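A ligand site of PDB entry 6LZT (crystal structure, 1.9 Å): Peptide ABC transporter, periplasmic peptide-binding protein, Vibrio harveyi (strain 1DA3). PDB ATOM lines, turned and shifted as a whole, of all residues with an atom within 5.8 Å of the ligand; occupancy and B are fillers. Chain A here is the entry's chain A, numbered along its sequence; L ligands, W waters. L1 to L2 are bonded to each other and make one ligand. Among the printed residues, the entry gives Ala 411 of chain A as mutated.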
ATOM      1  N   HIS A   9      17.525  12.494  13.206  1.00  0.00           N
ATOM      2  CA  HIS A   9      17.812  12.540  14.647  1.00  0.00           C
ATOM      3  C   HIS A   9      18.549  13.838  15.018  1.00  0.00           C
ATOM      4  O   HIS A   9      19.764  13.846  15.142  1.00  0.00           O
ATOM      5  CB  HIS A   9      18.660  11.326  15.049  1.00  0.00           C
ATOM      6  CG  HIS A   9      19.005  11.282  16.506  1.00  0.00           C
ATOM      7  ND1 HIS A   9      18.107  11.624  17.484  1.00  0.00           N
ATOM      8  CD2 HIS A   9      20.142  10.903  17.140  1.00  0.00           C
ATOM      9  CE1 HIS A   9      18.684  11.487  18.681  1.00  0.00           C
ATOM     10  NE2 HIS A   9      19.900  11.033  18.494  1.00  0.00           N
ATOM     11  N   PRO A  10      17.817  14.953  15.143  1.00  0.00           N
ATOM     12  CA  PRO A  10      18.512  16.226  15.351  1.00  0.00           C
ATOM     13  C   PRO A  10      18.900  16.478  16.812  1.00  0.00           C
ATOM     14  O   PRO A  10      19.792  17.303  17.080  1.00  0.00           O
ATOM     15  CB  PRO A  10      17.490  17.254  14.879  1.00  0.00           C
ATOM     16  CG  PRO A  10      16.183  16.617  15.187  1.00  0.00           C
ATOM     17  CD  PRO A  10      16.369  15.149  14.922  1.00  0.00           C
ATOM     18  N   LYS A  11      18.244  15.790  17.734  1.00  0.00           N
ATOM     19  CA  LYS A  11      18.407  16.102  19.166  1.00  0.00           C
ATOM     20  C   LYS A  11      17.968  14.946  20.050  1.00  0.00           C
ATOM     21  O   LYS A  11      16.914  14.347  19.821  1.00  0.00           O
ATOM     22  CB  LYS A  11      17.607  17.362  19.530  1.00  0.00           C
ATOM     23  CG  LYS A  11      17.607  17.739  21.006  1.00  0.00           C
ATOM     24  CD  LYS A  11      18.970  18.204  21.475  1.00  0.00           C
ATOM     25  CE  LYS A  11      18.938  18.557  22.965  1.00  0.00           C
ATOM     26  NZ  LYS A  11      18.042  19.734  23.177  1.00  0.00           N
ATOM     27  N   GLU A  12      18.772  14.642  21.055  1.00  0.00           N
ATOM     28  CA  GLU A  12      18.392  13.700  22.109  1.00  0.00           C
ATOM     29  C   GLU A  12      17.236  14.186  22.973  1.00  0.00           C
ATOM     30  O   GLU A  12      17.127  15.351  23.336  1.00  0.00           O
ATOM     31  CB  GLU A  12      19.593  13.398  23.008  1.00  0.00           C
ATOM     32  CG  GLU A  12      20.786  12.898  22.212  1.00  0.00           C
ATOM     33  CD  GLU A  12      21.804  14.000  21.968  1.00  0.00           C
ATOM     34  OE1 GLU A  12      21.407  15.182  21.761  1.00  0.00           O
ATOM     35  OE2 GLU A  12      23.019  13.688  21.994  1.00  0.00           O
ATOM     36  N   HIS A  30      13.299  19.920  17.729  1.00  0.00           N
ATOM     37  CA  HIS A  30      14.351  20.466  16.868  1.00  0.00           C
ATOM     38  C   HIS A  30      14.127  20.226  15.375  1.00  0.00           C
ATOM     39  O   HIS A  30      15.082  20.107  14.604  1.00  0.00           O
ATOM     40  CB  HIS A  30      15.731  19.921  17.240  1.00  0.00           C
ATOM     41  CG  HIS A  30      16.292  20.545  18.480  1.00  0.00           C
ATOM     42  ND1 HIS A  30      17.658  20.615  18.725  1.00  0.00           N
ATOM     43  CD2 HIS A  30      15.682  21.116  19.538  1.00  0.00           C
ATOM     44  CE1 HIS A  30      17.853  21.203  19.886  1.00  0.00           C
ATOM     45  NE2 HIS A  30      16.680  21.512  20.410  1.00  0.00           N
ATOM     46  N   ASN A 206      23.989   8.597  23.373  1.00  0.00           N
ATOM     47  CA  ASN A 206      24.787   8.020  22.289  1.00  0.00           C
ATOM     48  C   ASN A 206      24.798   6.496  22.180  1.00  0.00           C
ATOM     49  O   ASN A 206      24.968   5.943  21.098  1.00  0.00           O
ATOM     50  CB  ASN A 206      26.233   8.490  22.371  1.00  0.00           C
ATOM     51  CG  ASN A 206      26.419   9.887  21.844  1.00  0.00           C
ATOM     52  OD1 ASN A 206      25.502  10.448  21.233  1.00  0.00           O
ATOM     53  ND2 ASN A 206      27.593  10.457  22.058  1.00  0.00           N
ATOM     54  N   SER A 222      23.793  12.927  12.801  1.00  0.00           N
ATOM     55  CA  SER A 222      24.962  13.771  13.052  1.00  0.00           C
ATOM     56  C   SER A 222      25.519  13.500  14.465  1.00  0.00           C
ATOM     57  O   SER A 222      26.126  14.376  15.092  1.00  0.00           O
ATOM     58  CB  SER A 222      24.609  15.243  12.881  1.00  0.00           C
ATOM     59  OG  SER A 222      24.190  15.489  11.546  1.00  0.00           O
ATOM     60  N   SER A 223      25.300  12.298  14.964  1.00  0.00           N
ATOM     61  CA  SER A 223      25.737  11.943  16.326  1.00  0.00           C
ATOM     62  C   SER A 223      27.164  11.430  16.384  1.00  0.00           C
ATOM     63  O   SER A 223      27.735  11.034  15.375  1.00  0.00           O
ATOM     64  CB  SER A 223      24.786  10.892  16.902  1.00  0.00           C
ATOM     65  OG  SER A 223      23.557  11.469  17.296  1.00  0.00           O
ATOM     66  N   PHE A 224      27.755  11.421  17.582  1.00  0.00           N
ATOM     67  CA  PHE A 224      29.042  10.750  17.720  1.00  0.00           C
ATOM     68  C   PHE A 224      28.840   9.244  17.674  1.00  0.00           C
ATOM     69  O   PHE A 224      27.907   8.718  18.301  1.00  0.00           O
ATOM     70  CB  PHE A 224      29.748  11.140  19.026  1.00  0.00           C
ATOM     71  CG  PHE A 224      30.985  10.316  19.290  1.00  0.00           C
ATOM     72  CD1 PHE A 224      32.120  10.491  18.513  1.00  0.00           C
ATOM     73  CD2 PHE A 224      30.999   9.350  20.284  1.00  0.00           C
ATOM     74  CE1 PHE A 224      33.253   9.737  18.742  1.00  0.00           C
ATOM     75  CE2 PHE A 224      32.126   8.590  20.525  1.00  0.00           C
ATOM     76  CZ  PHE A 224      33.257   8.781  19.755  1.00  0.00           C
ATOM     77  N   GLN A 249      36.428  23.361  20.212  1.00  0.00           N
ATOM     78  CA  GLN A 249      35.950  22.791  21.458  1.00  0.00           C
ATOM     79  C   GLN A 249      36.930  23.214  22.539  1.00  0.00           C
ATOM     80  O   GLN A 249      38.143  23.206  22.307  1.00  0.00           O
ATOM     81  CB  GLN A 249      35.823  21.274  21.379  1.00  0.00           C
ATOM     82  CG  GLN A 249      34.923  20.820  20.239  1.00  0.00           C
ATOM     83  CD  GLN A 249      34.677  19.314  20.221  1.00  0.00           C
ATOM     84  OE1 GLN A 249      35.263  18.563  20.999  1.00  0.00           O
ATOM     85  NE2 GLN A 249      33.807  18.886  19.345  1.00  0.00           N
ATOM     86  N   PHE A 289      37.736  10.820  20.829  1.00  0.00           N
ATOM     87  CA  PHE A 289      37.105  11.041  19.526  1.00  0.00           C
ATOM     88  C   PHE A 289      37.562  10.064  18.452  1.00  0.00           C
ATOM     89  O   PHE A 289      37.148  10.167  17.306  1.00  0.00           O
ATOM     90  CB  PHE A 289      37.372  12.463  19.050  1.00  0.00           C
ATOM     91  CG  PHE A 289      36.744  13.513  19.909  1.00  0.00           C
ATOM     92  CD1 PHE A 289      35.408  13.843  19.767  1.00  0.00           C
ATOM     93  CD2 PHE A 289      37.498  14.192  20.861  1.00  0.00           C
ATOM     94  CE1 PHE A 289      34.833  14.804  20.558  1.00  0.00           C
ATOM     95  CE2 PHE A 289      36.920  15.169  21.659  1.00  0.00           C
ATOM     96  CZ  PHE A 289      35.587  15.480  21.501  1.00  0.00           C
ATOM     97  N   GLY A 364      24.922  11.866  28.067  1.00  0.00           N
ATOM     98  CA  GLY A 364      24.783  11.177  26.790  1.00  0.00           C
ATOM     99  C   GLY A 364      25.743  11.590  25.666  1.00  0.00           C
ATOM    100  O   GLY A 364      25.852  10.872  24.670  1.00  0.00           O
ATOM    101  N   TRP A 365      26.428  12.723  25.824  1.00  0.00           N
ATOM    102  CA  TRP A 365      27.415  13.169  24.839  1.00  0.00           C
ATOM    103  C   TRP A 365      28.738  12.473  25.119  1.00  0.00           C
ATOM    104  O   TRP A 365      29.669  13.112  25.619  1.00  0.00           O
ATOM    105  CB  TRP A 365      27.626  14.695  24.901  1.00  0.00           C
ATOM    106  CG  TRP A 365      26.425  15.496  24.522  1.00  0.00           C
ATOM    107  CD1 TRP A 365      25.122  15.094  24.558  1.00  0.00           C
ATOM    108  CD2 TRP A 365      26.418  16.842  24.035  1.00  0.00           C
ATOM    109  NE1 TRP A 365      24.310  16.100  24.126  1.00  0.00           N
ATOM    110  CE2 TRP A 365      25.074  17.186  23.807  1.00  0.00           C
ATOM    111  CE3 TRP A 365      27.419  17.791  23.786  1.00  0.00           C
ATOM    112  CZ2 TRP A 365      24.703  18.443  23.294  1.00  0.00           C
ATOM    113  CZ3 TRP A 365      27.048  19.042  23.306  1.00  0.00           C
ATOM    114  CH2 TRP A 365      25.697  19.349  23.055  1.00  0.00           C
ATOM    115  N   THR A 366      28.816  11.186  24.793  1.00  0.00           N
ATOM    116  CA  THR A 366      29.886  10.327  25.352  1.00  0.00           C
ATOM    117  C   THR A 366      31.289  10.792  24.968  1.00  0.00           C
ATOM    118  O   THR A 366      32.216  10.687  25.770  1.00  0.00           O
ATOM    119  CB  THR A 366      29.695   8.868  24.925  1.00  0.00           C
ATOM    120  OG1 THR A 366      29.591   8.802  23.491  1.00  0.00           O
ATOM    121  CG2 THR A 366      28.433   8.293  25.541  1.00  0.00           C
ATOM    122  N   ASP A 367      31.440  11.335  23.767  1.00  0.00           N
ATOM    123  CA  ASP A 367      32.734  11.860  23.341  1.00  0.00           C
ATOM    124  C   ASP A 367      33.178  13.011  24.261  1.00  0.00           C
ATOM    125  O   ASP A 367      34.333  13.068  24.679  1.00  0.00           O
ATOM    126  CB  ASP A 367      32.719  12.285  21.868  1.00  0.00           C
ATOM    127  CG  ASP A 367      31.493  13.103  21.483  1.00  0.00           C
ATOM    128  OD1 ASP A 367      30.453  12.990  22.148  1.00  0.00           O
ATOM    129  OD2 ASP A 367      31.570  13.838  20.478  1.00  0.00           O
ATOM    130  N   PHE A 368      32.249  13.898  24.603  1.00  0.00           N
ATOM    131  CA  PHE A 368      32.577  14.965  25.556  1.00  0.00           C
ATOM    132  C   PHE A 368      32.810  14.373  26.930  1.00  0.00           C
ATOM    133  O   PHE A 368      33.726  14.811  27.641  1.00  0.00           O
ATOM    134  CB  PHE A 368      31.482  16.034  25.615  1.00  0.00           C
ATOM    135  CG  PHE A 368      31.418  16.919  24.388  1.00  0.00           C
ATOM    136  CD1 PHE A 368      32.142  16.613  23.255  1.00  0.00           C
ATOM    137  CD2 PHE A 368      30.692  18.097  24.406  1.00  0.00           C
ATOM    138  CE1 PHE A 368      32.092  17.439  22.106  1.00  0.00           C
ATOM    139  CE2 PHE A 368      30.655  18.932  23.287  1.00  0.00           C
ATOM    140  CZ  PHE A 368      31.358  18.585  22.121  1.00  0.00           C
ATOM    141  N   THR A 410      32.676  22.542  26.100  1.00  0.00           N
ATOM    142  CA  THR A 410      31.697  22.789  25.045  1.00  0.00           C
ATOM    143  C   THR A 410      32.319  22.954  23.679  1.00  0.00           C
ATOM    144  O   THR A 410      33.486  23.326  23.548  1.00  0.00           O
ATOM    145  CB  THR A 410      30.857  24.048  25.314  1.00  0.00           C
ATOM    146  OG1 THR A 410      29.913  24.215  24.238  1.00  0.00           O
ATOM    147  CG2 THR A 410      31.758  25.280  25.371  1.00  0.00           C
ATOM    148  N   ALA A 411      31.523  22.661  22.672  1.00  0.00           N
ATOM    149  CA  ALA A 411      31.876  23.013  21.315  1.00  0.00           C
ATOM    150  C   ALA A 411      31.171  24.307  20.956  1.00  0.00           C
ATOM    151  O   ALA A 411      30.297  24.802  21.703  1.00  0.00           O
ATOM    152  CB  ALA A 411      31.504  21.913  20.346  1.00  0.00           C
ATOM    153  N   TYR A 412      31.555  24.864  19.809  1.00  0.00           N
ATOM    154  CA  TYR A 412      30.991  26.114  19.305  1.00  0.00           C
ATOM    155  C   TYR A 412      30.586  25.918  17.870  1.00  0.00           C
ATOM    156  O   TYR A 412      31.039  24.973  17.221  1.00  0.00           O
ATOM    157  CB  TYR A 412      31.999  27.257  19.381  1.00  0.00           C
ATOM    158  CG  TYR A 412      32.481  27.601  20.765  1.00  0.00           C
ATOM    159  CD1 TYR A 412      33.579  26.959  21.315  1.00  0.00           C
ATOM    160  CD2 TYR A 412      31.834  28.573  21.528  1.00  0.00           C
ATOM    161  CE1 TYR A 412      34.038  27.286  22.588  1.00  0.00           C
ATOM    162  CE2 TYR A 412      32.280  28.896  22.791  1.00  0.00           C
ATOM    163  CZ  TYR A 412      33.383  28.270  23.317  1.00  0.00           C
ATOM    164  OH  TYR A 412      33.829  28.632  24.591  1.00  0.00           O
ATOM    165  N   PHE A 413      29.759  26.818  17.350  1.00  0.00           N
ATOM    166  CA  PHE A 413      29.454  26.751  15.922  1.00  0.00           C
ATOM    167  C   PHE A 413      30.611  27.310  15.076  1.00  0.00           C
ATOM    168  O   PHE A 413      31.389  28.132  15.553  1.00  0.00           O
ATOM    169  CB  PHE A 413      28.136  27.463  15.618  1.00  0.00           C
ATOM    170  CG  PHE A 413      26.910  26.608  15.891  1.00  0.00           C
ATOM    171  CD1 PHE A 413      26.549  25.595  15.026  1.00  0.00           C
ATOM    172  CD2 PHE A 413      26.152  26.816  17.035  1.00  0.00           C
ATOM    173  CE1 PHE A 413      25.450  24.794  15.284  1.00  0.00           C
ATOM    174  CE2 PHE A 413      25.054  26.015  17.293  1.00  0.00           C
ATOM    175  CZ  PHE A 413      24.691  25.013  16.415  1.00  0.00           C
ATOM    176  N   ARG A 438      24.587  29.168  25.586  1.00  0.00           N
ATOM    177  CA  ARG A 438      25.543  29.050  26.702  1.00  0.00           C
ATOM    178  C   ARG A 438      26.936  29.603  26.410  1.00  0.00           C
ATOM    179  O   ARG A 438      27.751  29.714  27.327  1.00  0.00           O
ATOM    180  CB  ARG A 438      25.703  27.585  27.084  1.00  0.00           C
ATOM    181  CG  ARG A 438      26.405  26.773  25.977  1.00  0.00           C
ATOM    182  CD  ARG A 438      26.219  25.297  26.214  1.00  0.00           C
ATOM    183  NE  ARG A 438      26.815  24.462  25.178  1.00  0.00           N
ATOM    184  CZ  ARG A 438      26.233  24.160  24.024  1.00  0.00           C
ATOM    185  NH1 ARG A 438      25.030  24.655  23.749  1.00  0.00           N
ATOM    186  NH2 ARG A 438      26.846  23.367  23.144  1.00  0.00           N
ATOM    187  N   PHE A 439      27.203  29.937  25.153  1.00  0.00           N
ATOM    188  CA  PHE A 439      28.580  29.993  24.629  1.00  0.00           C
ATOM    189  C   PHE A 439      29.452  31.079  25.275  1.00  0.00           C
ATOM    190  O   PHE A 439      30.632  30.854  25.494  1.00  0.00           O
ATOM    191  CB  PHE A 439      28.538  30.164  23.101  1.00  0.00           C
ATOM    192  CG  PHE A 439      27.769  29.076  22.379  1.00  0.00           C
ATOM    193  CD1 PHE A 439      28.200  27.760  22.415  1.00  0.00           C
ATOM    194  CD2 PHE A 439      26.627  29.378  21.650  1.00  0.00           C
ATOM    195  CE1 PHE A 439      27.486  26.758  21.770  1.00  0.00           C
ATOM    196  CE2 PHE A 439      25.908  28.404  20.997  1.00  0.00           C
ATOM    197  CZ  PHE A 439      26.338  27.090  21.043  1.00  0.00           C
ATOM    198  N   MET A 491      30.071  15.886  12.514  1.00  0.00           N
ATOM    199  CA  MET A 491      29.659  14.484  12.459  1.00  0.00           C
ATOM    200  C   MET A 491      28.395  14.379  11.623  1.00  0.00           C
ATOM    201  O   MET A 491      27.459  15.171  11.770  1.00  0.00           O
ATOM    202  CB  MET A 491      29.410  13.976  13.862  1.00  0.00           C
ATOM    203  CG  MET A 491      30.390  14.628  14.826  1.00  0.00           C
ATOM    204  SD  MET A 491      29.603  14.840  16.420  1.00  0.00           S
ATOM    205  CE  MET A 491      30.390  16.371  16.893  1.00  0.00           C
ATOM    206  N   TRP A 515      21.284  18.865  12.709  1.00  0.00           N
ATOM    207  CA  TRP A 515      21.017  19.675  13.909  1.00  0.00           C
ATOM    208  C   TRP A 515      20.211  20.946  13.703  1.00  0.00           C
ATOM    209  O   TRP A 515      20.403  21.675  12.717  1.00  0.00           O
ATOM    210  CB  TRP A 515      22.338  20.107  14.568  1.00  0.00           C
ATOM    211  CG  TRP A 515      23.276  19.034  15.004  1.00  0.00           C
ATOM    212  CD1 TRP A 515      22.962  17.770  15.408  1.00  0.00           C
ATOM    213  CD2 TRP A 515      24.707  19.131  15.050  1.00  0.00           C
ATOM    214  NE1 TRP A 515      24.110  17.087  15.734  1.00  0.00           N
ATOM    215  CE2 TRP A 515      25.192  17.892  15.504  1.00  0.00           C
ATOM    216  CE3 TRP A 515      25.618  20.151  14.757  1.00  0.00           C
ATOM    217  CZ2 TRP A 515      26.558  17.635  15.682  1.00  0.00           C
ATOM    218  CZ3 TRP A 515      26.985  19.892  14.926  1.00  0.00           C
ATOM    219  CH2 TRP A 515      27.441  18.650  15.388  1.00  0.00           C
ATOM    220  N   ALA A 516      19.356  21.291  14.663  1.00  0.00           N
ATOM    221  CA  ALA A 516      18.846  22.671  14.730  1.00  0.00           C
ATOM    222  C   ALA A 516      20.012  23.694  14.784  1.00  0.00           C
ATOM    223  O   ALA A 516      21.031  23.455  15.438  1.00  0.00           O
ATOM    224  CB  ALA A 516      17.906  22.846  15.921  1.00  0.00           C
HETATM  225  C1  LIG L   1      24.026  21.029  18.887  1.00  0.00           C
HETATM  226  C2  LIG L   1      25.463  20.807  19.392  1.00  0.00           C
HETATM  227  C3  LIG L   1      25.866  19.393  18.996  1.00  0.00           C
HETATM  228  C4  LIG L   1      24.824  18.358  19.428  1.00  0.00           C
HETATM  229  C5  LIG L   1      23.428  18.793  19.009  1.00  0.00           C
HETATM  230  C6  LIG L   1      22.371  17.799  19.471  1.00  0.00           C
HETATM  231  C7  LIG L   1      26.856  22.835  19.335  1.00  0.00           C
HETATM  232  C8  LIG L   1      27.696  23.739  18.477  1.00  0.00           C
HETATM  233  N1  LIG L   1      26.417  21.721  18.766  1.00  0.00           N
HETATM  234  O1  LIG L   1      23.508  22.347  19.123  1.00  0.00           O
HETATM  235  O2  LIG L   1      27.145  19.115  19.585  1.00  0.00           O
HETATM  236  O3  LIG L   1      25.087  17.088  18.843  1.00  0.00           O
HETATM  237  O4  LIG L   1      23.162  20.094  19.545  1.00  0.00           O
HETATM  238  O5  LIG L   1      22.469  17.692  20.895  1.00  0.00           O
HETATM  239  O6  LIG L   1      26.616  23.115  20.488  1.00  0.00           O
HETATM  240  C1  LG2 L   2      25.586  16.143  19.784  1.00  0.00           C
HETATM  241  C2  LG2 L   2      25.283  14.713  19.342  1.00  0.00           C
HETATM  242  C3  LG2 L   2      25.957  13.747  20.321  1.00  0.00           C
HETATM  243  C4  LG2 L   2      27.419  14.070  20.481  1.00  0.00           C
HETATM  244  C5  LG2 L   2      27.559  15.537  20.882  1.00  0.00           C
HETATM  245  C6  LG2 L   2      28.991  15.980  21.103  1.00  0.00           C
HETATM  246  C7  LG2 L   2      23.111  14.517  18.206  1.00  0.00           C
HETATM  247  C8  LG2 L   2      21.621  14.343  18.390  1.00  0.00           C
HETATM  248  N1  LG2 L   2      23.835  14.495  19.324  1.00  0.00           N
HETATM  249  O1  LG2 L   2      25.928  12.406  19.816  1.00  0.00           O
HETATM  250  O2  LG2 L   2      28.016  13.179  21.426  1.00  0.00           O
HETATM  251  O3  LG2 L   2      26.985  16.344  19.855  1.00  0.00           O
HETATM  252  O4  LG2 L   2      29.859  15.750  20.003  1.00  0.00           O
HETATM  253  O5  LG2 L   2      23.636  14.655  17.117  1.00  0.00           O
HETATM  254  O   HOH W   1      29.486  20.108  18.667  1.00  0.00           O
HETATM  255  O   HOH W   2      21.219  22.377  17.729  1.00  0.00           O
HETATM  256  O   HOH W   3      23.730  23.916  21.000  1.00  0.00           O
HETATM  257  O   HOH W   4      22.240  13.066  15.482  1.00  0.00           O
HETATM  258  O   HOH W   5      28.680  21.596  21.831  1.00  0.00           O
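The side-chain amide nitrogen of Asn 206 is in hydrogen-bond range of the side-chain hydroxyl of Thr 366, at 3.0 Å. The side-chain amide nitrogen of Asn 206 lies close to the backbone carbonyl oxygen of Gly 364 (3.2 Å). NE of Arg 438 sits at hydrogen-bond distance from OG1 of Thr 410, 3.2 Å away. The indole nitrogen (NE1) of Trp 515 lies close to the backbone carbonyl oxygen (O) of Ser 222, 3.4 Å away. The side-chain carboxylate of Glu 12 sits at hydrogen-bond distance from the indole nitrogen of Trp 365, at 3.5 Å. The backbone carbonyl oxygen of Met 491 sits close to the side-chain hydroxyl of Ser 222 (3.3 Å).
Water W3 bridges O1 of LIG L1 and NH1 of Arg 438. Water W4 lies within hydrogen-bond range of O of His 9, O5 of LG2 L2, OG of Ser 223 and N of Ser 222. Water W2 lies within hydrogen-bond range of the backbone carbonyl oxygen (O) of Ala 516 (2.5 Å) and an oxygen (O1) of LIG L1 (2.7 Å). Water W5 lies within hydrogen-bond range of NH2 of Arg 438 (2.9 Å), O6 of LIG L1 (2.9 Å) and N of Ala 411 (3.2 Å).
The backbone carbonyl oxygen (O) of Ser 222 sits close to an oxygen (O5) of LG2 L2, at 3.2 Å. Merely in contact with the ligand: His 9, Pro 10, Lys 11, Trp 365, Thr 366, Phe 368, Tyr 412, Phe 413 and Phe 439. Hydrophobic or aromatic side chains that line the ligand: His 9, Phe 224, Trp 365, Phe 368, Phe 413, Phe 439, Met 491 and Trp 515. The nearest printed residue that does not touch the ligand is Ala 411 (4.2 Å).
The side-chain amide oxygen (OD1) of Asn 206 sits at hydrogen-bond distance from an oxygen (O1) of LG2 L2, 2.5 Å away. The side-chain carboxylate (OD1) of Asp 367 is in hydrogen-bond range of an oxygen (O2) of LG2 L2, at 2.5 Å. NH2 of Arg 438 sits at hydrogen-bond distance from O6 of LIG L1, 2.7 Å away. An oxygen (O5) of LG2 L2 lies within hydrogen-bond range of the indole nitrogen of Trp 515 (2.8 Å). The side-chain carboxylate of Glu 12 lies within hydrogen-bond range of an oxygen (O5) of LIG L1 (2.9 Å). O1 of LG2 L2 sits at hydrogen-bond distance from N of Phe 224 (3.0 Å). OG of Ser 223 lies within hydrogen-bond range of O5 of LG2 L2 (3.2 Å). An oxygen (O4) of LG2 L2 sits close to the side-chain sulfur (SD) of Met 491 (3.7 Å).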
